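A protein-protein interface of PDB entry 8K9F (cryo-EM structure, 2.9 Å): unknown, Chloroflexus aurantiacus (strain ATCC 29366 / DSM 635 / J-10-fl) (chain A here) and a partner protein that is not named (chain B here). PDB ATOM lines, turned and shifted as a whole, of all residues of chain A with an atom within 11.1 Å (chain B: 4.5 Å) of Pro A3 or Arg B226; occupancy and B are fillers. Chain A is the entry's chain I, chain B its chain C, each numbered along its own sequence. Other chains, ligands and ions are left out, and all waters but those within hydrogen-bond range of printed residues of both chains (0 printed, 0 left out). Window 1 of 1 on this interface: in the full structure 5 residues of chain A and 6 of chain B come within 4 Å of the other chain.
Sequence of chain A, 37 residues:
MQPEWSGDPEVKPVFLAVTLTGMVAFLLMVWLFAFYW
Pro A3 touches one residue of chain B.
Arg B226 touches just these residues of chain A: Met A1 (3.7 Å), Gln A2 (2.9 Å) and Pro A3 (3.5 Å).
His B225 touches just one residue of chain A: Met A1 (2.8 Å).
No residue of chain A comes within 4 Å of Met B229.
Of the printed residues of chain B, Met A1 touches Arg B222, His B225 and Arg B226.
Of the printed residues of chain B, Glu A4 touches His B223.
Printed residues of chain A within 4 Å of Arg B222: Met A1.
Of the printed residues of chain B, Gln A2 touches Arg B226.
The nearest printed residue of chain B that does not touch Pro A3 is Arg B222 (7.1 Å).
The nearest residue of chain A that does not touch Arg B226 is Glu A4 (5.1 Å).
The nearest printed residue of chain B that does not touch Gln A2 is Arg B222 (5.6 Å).
The backbone carbonyl oxygen of Gln A2 sits at hydrogen-bond distance from the guanidinium group of Arg B226, at 2.9 Å.
A ring nitrogen (NE2) of His B223 lies within hydrogen-bond range of the side-chain carboxylate of Glu A4 (3.1 Å).
The side-chain sulfur (SD) of Met A1 lies within hydrogen-bond range of a ring nitrogen (ND1) of His B225 (2.8 Å).
The guanidinium group (NH2) of Arg B226 lies close to the backbone nitrogen (N) of Pro A3 (3.5 Å).
NH1 of Arg B226 sits at hydrogen-bond distance from O of Arg B222 (2.8 Å).
The backbone carbonyl oxygen (O) of Pro A3 is in hydrogen-bond range of the side-chain hydroxyl (OG) of Ser A6, at 2.6 Å.
Of the 11 printed residues of chain A, 4 touch a printed residue of chain B.
Hydrophobic or aromatic side chains of chain A within 4 Å of the printed part of chain B: Met A1.
Among the printed residues, no Asp or Glu carboxylate lies within 4 Å of a Lys or Arg side-chain nitrogen of the other chain.
Among the printed residues, pairs that only touch across the chains: Met A1 with Arg B222 and Met A1 with Arg B226.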
ATOM      1  N   MET A   1      25.349   6.216  -8.981  1.00  0.00           N
ATOM      2  CA  MET A   1      24.757   6.876  -7.824  1.00  0.00           C
ATOM      3  C   MET A   1      24.578   5.912  -6.666  1.00  0.00           C
ATOM      4  O   MET A   1      24.296   4.729  -6.856  1.00  0.00           O
ATOM      5  CB  MET A   1      23.401   7.490  -8.177  1.00  0.00           C
ATOM      6  CG  MET A   1      23.469   8.812  -8.920  1.00  0.00           C
ATOM      7  SD  MET A   1      21.892   9.351  -9.621  1.00  0.00           S
ATOM      8  CE  MET A   1      20.705   8.363  -8.716  1.00  0.00           C
ATOM      9  N   GLN A   2      24.731   6.435  -5.463  1.00  0.00           N
ATOM     10  CA  GLN A   2      24.467   5.716  -4.231  1.00  0.00           C
ATOM     11  C   GLN A   2      23.263   6.350  -3.559  1.00  0.00           C
ATOM     12  O   GLN A   2      22.927   7.506  -3.839  1.00  0.00           O
ATOM     13  CB  GLN A   2      25.688   5.745  -3.296  1.00  0.00           C
ATOM     14  CG  GLN A   2      26.527   7.007  -3.369  1.00  0.00           C
ATOM     15  CD  GLN A   2      27.837   6.862  -2.621  1.00  0.00           C
ATOM     16  OE1 GLN A   2      28.353   5.757  -2.460  1.00  0.00           O
ATOM     17  NE2 GLN A   2      28.381   7.979  -2.155  1.00  0.00           N
ATOM     18  N   PRO A   3      22.556   5.605  -2.702  1.00  0.00           N
ATOM     19  CA  PRO A   3      21.500   6.226  -1.892  1.00  0.00           C
ATOM     20  C   PRO A   3      22.060   7.215  -0.887  1.00  0.00           C
ATOM     21  O   PRO A   3      23.251   7.177  -0.568  1.00  0.00           O
ATOM     22  CB  PRO A   3      20.846   5.033  -1.186  1.00  0.00           C
ATOM     23  CG  PRO A   3      21.852   3.936  -1.282  1.00  0.00           C
ATOM     24  CD  PRO A   3      22.543   4.138  -2.573  1.00  0.00           C
ATOM     25  N   GLU A   4      21.217   8.107  -0.378  1.00  0.00           N
ATOM     26  CA  GLU A   4      21.687   9.091   0.584  1.00  0.00           C
ATOM     27  C   GLU A   4      21.820   8.533   1.992  1.00  0.00           C
ATOM     28  O   GLU A   4      22.357   9.221   2.866  1.00  0.00           O
ATOM     29  CB  GLU A   4      20.756  10.300   0.610  1.00  0.00           C
ATOM     30  CG  GLU A   4      19.470  10.077   1.359  1.00  0.00           C
ATOM     31  CD  GLU A   4      18.393  11.021   0.900  1.00  0.00           C
ATOM     32  OE1 GLU A   4      18.540  11.584  -0.206  1.00  0.00           O
ATOM     33  OE2 GLU A   4      17.400  11.209   1.639  1.00  0.00           O
ATOM     34  N   TRP A   5      21.343   7.316   2.240  1.00  0.00           N
ATOM     35  CA  TRP A   5      21.550   6.658   3.519  1.00  0.00           C
ATOM     36  C   TRP A   5      22.667   5.627   3.458  1.00  0.00           C
ATOM     37  O   TRP A   5      22.786   4.798   4.364  1.00  0.00           O
ATOM     38  CB  TRP A   5      20.244   6.026   4.006  1.00  0.00           C
ATOM     39  CG  TRP A   5      19.401   5.389   2.942  1.00  0.00           C
ATOM     40  CD1 TRP A   5      18.197   5.834   2.493  1.00  0.00           C
ATOM     41  CD2 TRP A   5      19.640   4.143   2.271  1.00  0.00           C
ATOM     42  NE1 TRP A   5      17.699   4.980   1.549  1.00  0.00           N
ATOM     43  CE2 TRP A   5      18.562   3.928   1.400  1.00  0.00           C
ATOM     44  CE3 TRP A   5      20.670   3.202   2.308  1.00  0.00           C
ATOM     45  CZ2 TRP A   5      18.487   2.816   0.570  1.00  0.00           C
ATOM     46  CZ3 TRP A   5      20.590   2.098   1.495  1.00  0.00           C
ATOM     47  CH2 TRP A   5      19.508   1.913   0.632  1.00  0.00           C
ATOM     48  N   SER A   6      23.473   5.654   2.391  1.00  0.00           N
ATOM     49  CA  SER A   6      24.558   4.690   2.237  1.00  0.00           C
ATOM     50  C   SER A   6      25.658   4.904   3.268  1.00  0.00           C
ATOM     51  O   SER A   6      26.210   3.931   3.795  1.00  0.00           O
ATOM     52  CB  SER A   6      25.145   4.782   0.830  1.00  0.00           C
ATOM     53  OG  SER A   6      25.411   6.128   0.485  1.00  0.00           O
ATOM     54  N   GLY A   7      25.982   6.157   3.569  1.00  0.00           N
ATOM     55  CA  GLY A   7      27.019   6.458   4.531  1.00  0.00           C
ATOM     56  C   GLY A   7      26.471   6.913   5.865  1.00  0.00           C
ATOM     57  O   GLY A   7      27.006   7.838   6.482  1.00  0.00           O
ATOM     58  N   ASP A   8      25.397   6.276   6.314  1.00  0.00           N
ATOM     59  CA  ASP A   8      24.797   6.615   7.590  1.00  0.00           C
ATOM     60  C   ASP A   8      24.986   5.474   8.580  1.00  0.00           C
ATOM     61  O   ASP A   8      24.951   4.305   8.183  1.00  0.00           O
ATOM     62  CB  ASP A   8      23.301   6.907   7.439  1.00  0.00           C
ATOM     63  CG  ASP A   8      23.030   8.214   6.722  1.00  0.00           C
ATOM     64  OD1 ASP A   8      23.967   9.032   6.590  1.00  0.00           O
ATOM     65  OD2 ASP A   8      21.876   8.426   6.291  1.00  0.00           O
ATOM     66  N   PRO A   9      25.204   5.778   9.864  1.00  0.00           N
ATOM     67  CA  PRO A   9      25.317   4.702  10.864  1.00  0.00           C
ATOM     68  C   PRO A   9      24.023   3.941  11.095  1.00  0.00           C
ATOM     69  O   PRO A   9      24.069   2.822  11.621  1.00  0.00           O
ATOM     70  CB  PRO A   9      25.759   5.447  12.133  1.00  0.00           C
ATOM     71  CG  PRO A   9      26.366   6.731  11.626  1.00  0.00           C
ATOM     72  CD  PRO A   9      25.507   7.094  10.449  1.00  0.00           C
ATOM     73  N   VAL A  11      22.233   2.664   8.746  1.00  0.00           N
ATOM     74  CA  VAL A  11      21.978   1.714   7.667  1.00  0.00           C
ATOM     75  C   VAL A  11      22.284   0.275   8.077  1.00  0.00           C
ATOM     76  O   VAL A  11      21.726  -0.661   7.491  1.00  0.00           O
ATOM     77  CB  VAL A  11      22.749   2.115   6.387  1.00  0.00           C
ATOM     78  CG1 VAL A  11      24.194   1.629   6.398  1.00  0.00           C
ATOM     79  CG2 VAL A  11      22.036   1.594   5.159  1.00  0.00           C
ATOM     80  N   PHE A  15      18.535  -2.006   8.537  1.00  0.00           N
ATOM     81  CA  PHE A  15      18.400  -3.096   7.579  1.00  0.00           C
ATOM     82  C   PHE A  15      18.610  -4.458   8.225  1.00  0.00           C
ATOM     83  O   PHE A  15      18.212  -5.470   7.643  1.00  0.00           O
ATOM     84  CB  PHE A  15      19.355  -2.903   6.405  1.00  0.00           C
ATOM     85  CG  PHE A  15      18.784  -2.062   5.305  1.00  0.00           C
ATOM     86  CD1 PHE A  15      17.730  -2.534   4.533  1.00  0.00           C
ATOM     87  CD2 PHE A  15      19.284  -0.797   5.047  1.00  0.00           C
ATOM     88  CE1 PHE A  15      17.194  -1.765   3.523  1.00  0.00           C
ATOM     89  CE2 PHE A  15      18.749  -0.022   4.032  1.00  0.00           C
ATOM     90  CZ  PHE A  15      17.704  -0.507   3.272  1.00  0.00           C
ATOM     91  N   ARG B 222      19.628  13.486  -8.427  1.00  0.00           N
ATOM     92  CA  ARG B 222      19.816  12.256  -7.638  1.00  0.00           C
ATOM     93  C   ARG B 222      18.505  11.793  -7.000  1.00  0.00           C
ATOM     94  O   ARG B 222      18.449  10.713  -6.405  1.00  0.00           O
ATOM     95  CB  ARG B 222      20.914  12.389  -6.563  1.00  0.00           C
ATOM     96  CG  ARG B 222      22.328  12.092  -7.029  1.00  0.00           C
ATOM     97  CD  ARG B 222      23.323  13.102  -6.463  1.00  0.00           C
ATOM     98  NE  ARG B 222      23.065  13.421  -5.063  1.00  0.00           N
ATOM     99  CZ  ARG B 222      23.850  14.180  -4.311  1.00  0.00           C
ATOM    100  NH1 ARG B 222      24.971  14.700  -4.783  1.00  0.00           N
ATOM    101  NH2 ARG B 222      23.502  14.423  -3.051  1.00  0.00           N
ATOM    102  N   HIS B 223      17.452  12.594  -7.120  1.00  0.00           N
ATOM    103  CA  HIS B 223      16.070  12.214  -6.878  1.00  0.00           C
ATOM    104  C   HIS B 223      15.261  12.196  -8.160  1.00  0.00           C
ATOM    105  O   HIS B 223      14.416  11.321  -8.341  1.00  0.00           O
ATOM    106  CB  HIS B 223      15.408  13.184  -5.898  1.00  0.00           C
ATOM    107  CG  HIS B 223      15.784  12.962  -4.470  1.00  0.00           C
ATOM    108  ND1 HIS B 223      14.935  13.262  -3.430  1.00  0.00           N
ATOM    109  CD2 HIS B 223      16.915  12.480  -3.907  1.00  0.00           C
ATOM    110  CE1 HIS B 223      15.526  12.971  -2.287  1.00  0.00           C
ATOM    111  NE2 HIS B 223      16.729  12.495  -2.548  1.00  0.00           N
ATOM    112  N   TRP B 224      15.505  13.160  -9.050  1.00  0.00           N
ATOM    113  CA  TRP B 224      14.881  13.143 -10.364  1.00  0.00           C
ATOM    114  C   TRP B 224      15.463  12.061 -11.254  1.00  0.00           C
ATOM    115  O   TRP B 224      14.771  11.594 -12.161  1.00  0.00           O
ATOM    116  CB  TRP B 224      15.034  14.489 -11.074  1.00  0.00           C
ATOM    117  CG  TRP B 224      14.105  15.594 -10.645  1.00  0.00           C
ATOM    118  CD1 TRP B 224      14.473  16.839 -10.255  1.00  0.00           C
ATOM    119  CD2 TRP B 224      12.667  15.573 -10.601  1.00  0.00           C
ATOM    120  NE1 TRP B 224      13.372  17.592  -9.955  1.00  0.00           N
ATOM    121  CE2 TRP B 224      12.251  16.839 -10.163  1.00  0.00           C
ATOM    122  CE3 TRP B 224      11.694  14.604 -10.875  1.00  0.00           C
ATOM    123  CZ2 TRP B 224      10.913  17.165  -9.996  1.00  0.00           C
ATOM    124  CZ3 TRP B 224      10.369  14.937 -10.727  1.00  0.00           C
ATOM    125  CH2 TRP B 224       9.989  16.203 -10.283  1.00  0.00           C
ATOM    126  N   HIS B 225      16.729  11.682 -11.040  1.00  0.00           N
ATOM    127  CA  HIS B 225      17.326  10.592 -11.809  1.00  0.00           C
ATOM    128  C   HIS B 225      16.586   9.294 -11.543  1.00  0.00           C
ATOM    129  O   HIS B 225      16.140   8.609 -12.471  1.00  0.00           O
ATOM    130  CB  HIS B 225      18.797  10.430 -11.441  1.00  0.00           C
ATOM    131  CG  HIS B 225      19.601   9.723 -12.487  1.00  0.00           C
ATOM    132  ND1 HIS B 225      20.861   9.222 -12.247  1.00  0.00           N
ATOM    133  CD2 HIS B 225      19.334   9.464 -13.788  1.00  0.00           C
ATOM    134  CE1 HIS B 225      21.329   8.672 -13.353  1.00  0.00           C
ATOM    135  NE2 HIS B 225      20.422   8.807 -14.303  1.00  0.00           N
ATOM    136  N   ARG B 226      16.388   8.987 -10.262  1.00  0.00           N
ATOM    137  CA  ARG B 226      15.594   7.836  -9.876  1.00  0.00           C
ATOM    138  C   ARG B 226      14.129   8.026 -10.229  1.00  0.00           C
ATOM    139  O   ARG B 226      13.438   7.036 -10.482  1.00  0.00           O
ATOM    140  CB  ARG B 226      15.774   7.571  -8.386  1.00  0.00           C
ATOM    141  CG  ARG B 226      17.197   7.170  -8.049  1.00  0.00           C
ATOM    142  CD  ARG B 226      17.272   6.295  -6.820  1.00  0.00           C
ATOM    143  NE  ARG B 226      18.642   6.156  -6.342  1.00  0.00           N
ATOM    144  CZ  ARG B 226      19.287   7.059  -5.614  1.00  0.00           C
ATOM    145  NH1 ARG B 226      18.721   8.200  -5.260  1.00  0.00           N
ATOM    146  NH2 ARG B 226      20.534   6.810  -5.235  1.00  0.00           N
ATOM    147  N   TYR B 227      13.656   9.275 -10.322  1.00  0.00           N
ATOM    148  CA  TYR B 227      12.284   9.504 -10.764  1.00  0.00           C
ATOM    149  C   TYR B 227      12.074   9.082 -12.210  1.00  0.00           C
ATOM    150  O   TYR B 227      11.172   8.285 -12.490  1.00  0.00           O
ATOM    151  CB  TYR B 227      11.857  10.964 -10.601  1.00  0.00           C
ATOM    152  CG  TYR B 227      10.357  11.050 -10.710  1.00  0.00           C
ATOM    153  CD1 TYR B 227       9.573  10.863  -9.600  1.00  0.00           C
ATOM    154  CD2 TYR B 227       9.722  11.269 -11.933  1.00  0.00           C
ATOM    155  CE1 TYR B 227       8.241  10.881  -9.678  1.00  0.00           C
ATOM    156  CE2 TYR B 227       8.379  11.274 -12.023  1.00  0.00           C
ATOM    157  CZ  TYR B 227       7.644  11.097 -10.886  1.00  0.00           C
ATOM    158  OH  TYR B 227       6.290  11.118 -10.943  1.00  0.00           O
ATOM    159  N   GLU B 228      12.837   9.666 -13.149  1.00  0.00           N
ATOM    160  CA  GLU B 228      12.688   9.287 -14.555  1.00  0.00           C
ATOM    161  C   GLU B 228      13.015   7.827 -14.760  1.00  0.00           C
ATOM    162  O   GLU B 228      12.400   7.160 -15.596  1.00  0.00           O
ATOM    163  CB  GLU B 228      13.580  10.118 -15.477  1.00  0.00           C
ATOM    164  CG  GLU B 228      13.692  11.563 -15.176  1.00  0.00           C
ATOM    165  CD  GLU B 228      12.492  12.310 -15.681  1.00  0.00           C
ATOM    166  OE1 GLU B 228      12.578  12.864 -16.796  1.00  0.00           O
ATOM    167  OE2 GLU B 228      11.467  12.352 -14.969  1.00  0.00           O
ATOM    168  N   MET B 229      13.933   7.312 -13.955  1.00  0.00           N
ATOM    169  CA  MET B 229      14.451   5.984 -14.168  1.00  0.00           C
ATOM    170  C   MET B 229      13.367   4.979 -13.772  1.00  0.00           C
ATOM    171  O   MET B 229      13.002   4.094 -14.560  1.00  0.00           O
ATOM    172  CB  MET B 229      15.682   5.887 -13.271  1.00  0.00           C
ATOM    173  CG  MET B 229      16.033   4.599 -12.667  1.00  0.00           C
ATOM    174  SD  MET B 229      16.270   3.453 -14.012  1.00  0.00           S
ATOM    175  CE  MET B 229      17.681   4.348 -14.700  1.00  0.00           C
ATOM    176  N   ALA B 230      12.765   5.186 -12.592  1.00  0.00           N
ATOM    177  CA  ALA B 230      11.687   4.345 -12.103  1.00  0.00           C
ATOM    178  C   ALA B 230      10.403   4.547 -12.884  1.00  0.00           C
ATOM    179  O   ALA B 230       9.636   3.601 -13.034  1.00  0.00           O
ATOM    180  CB  ALA B 230      11.438   4.622 -10.625  1.00  0.00           C
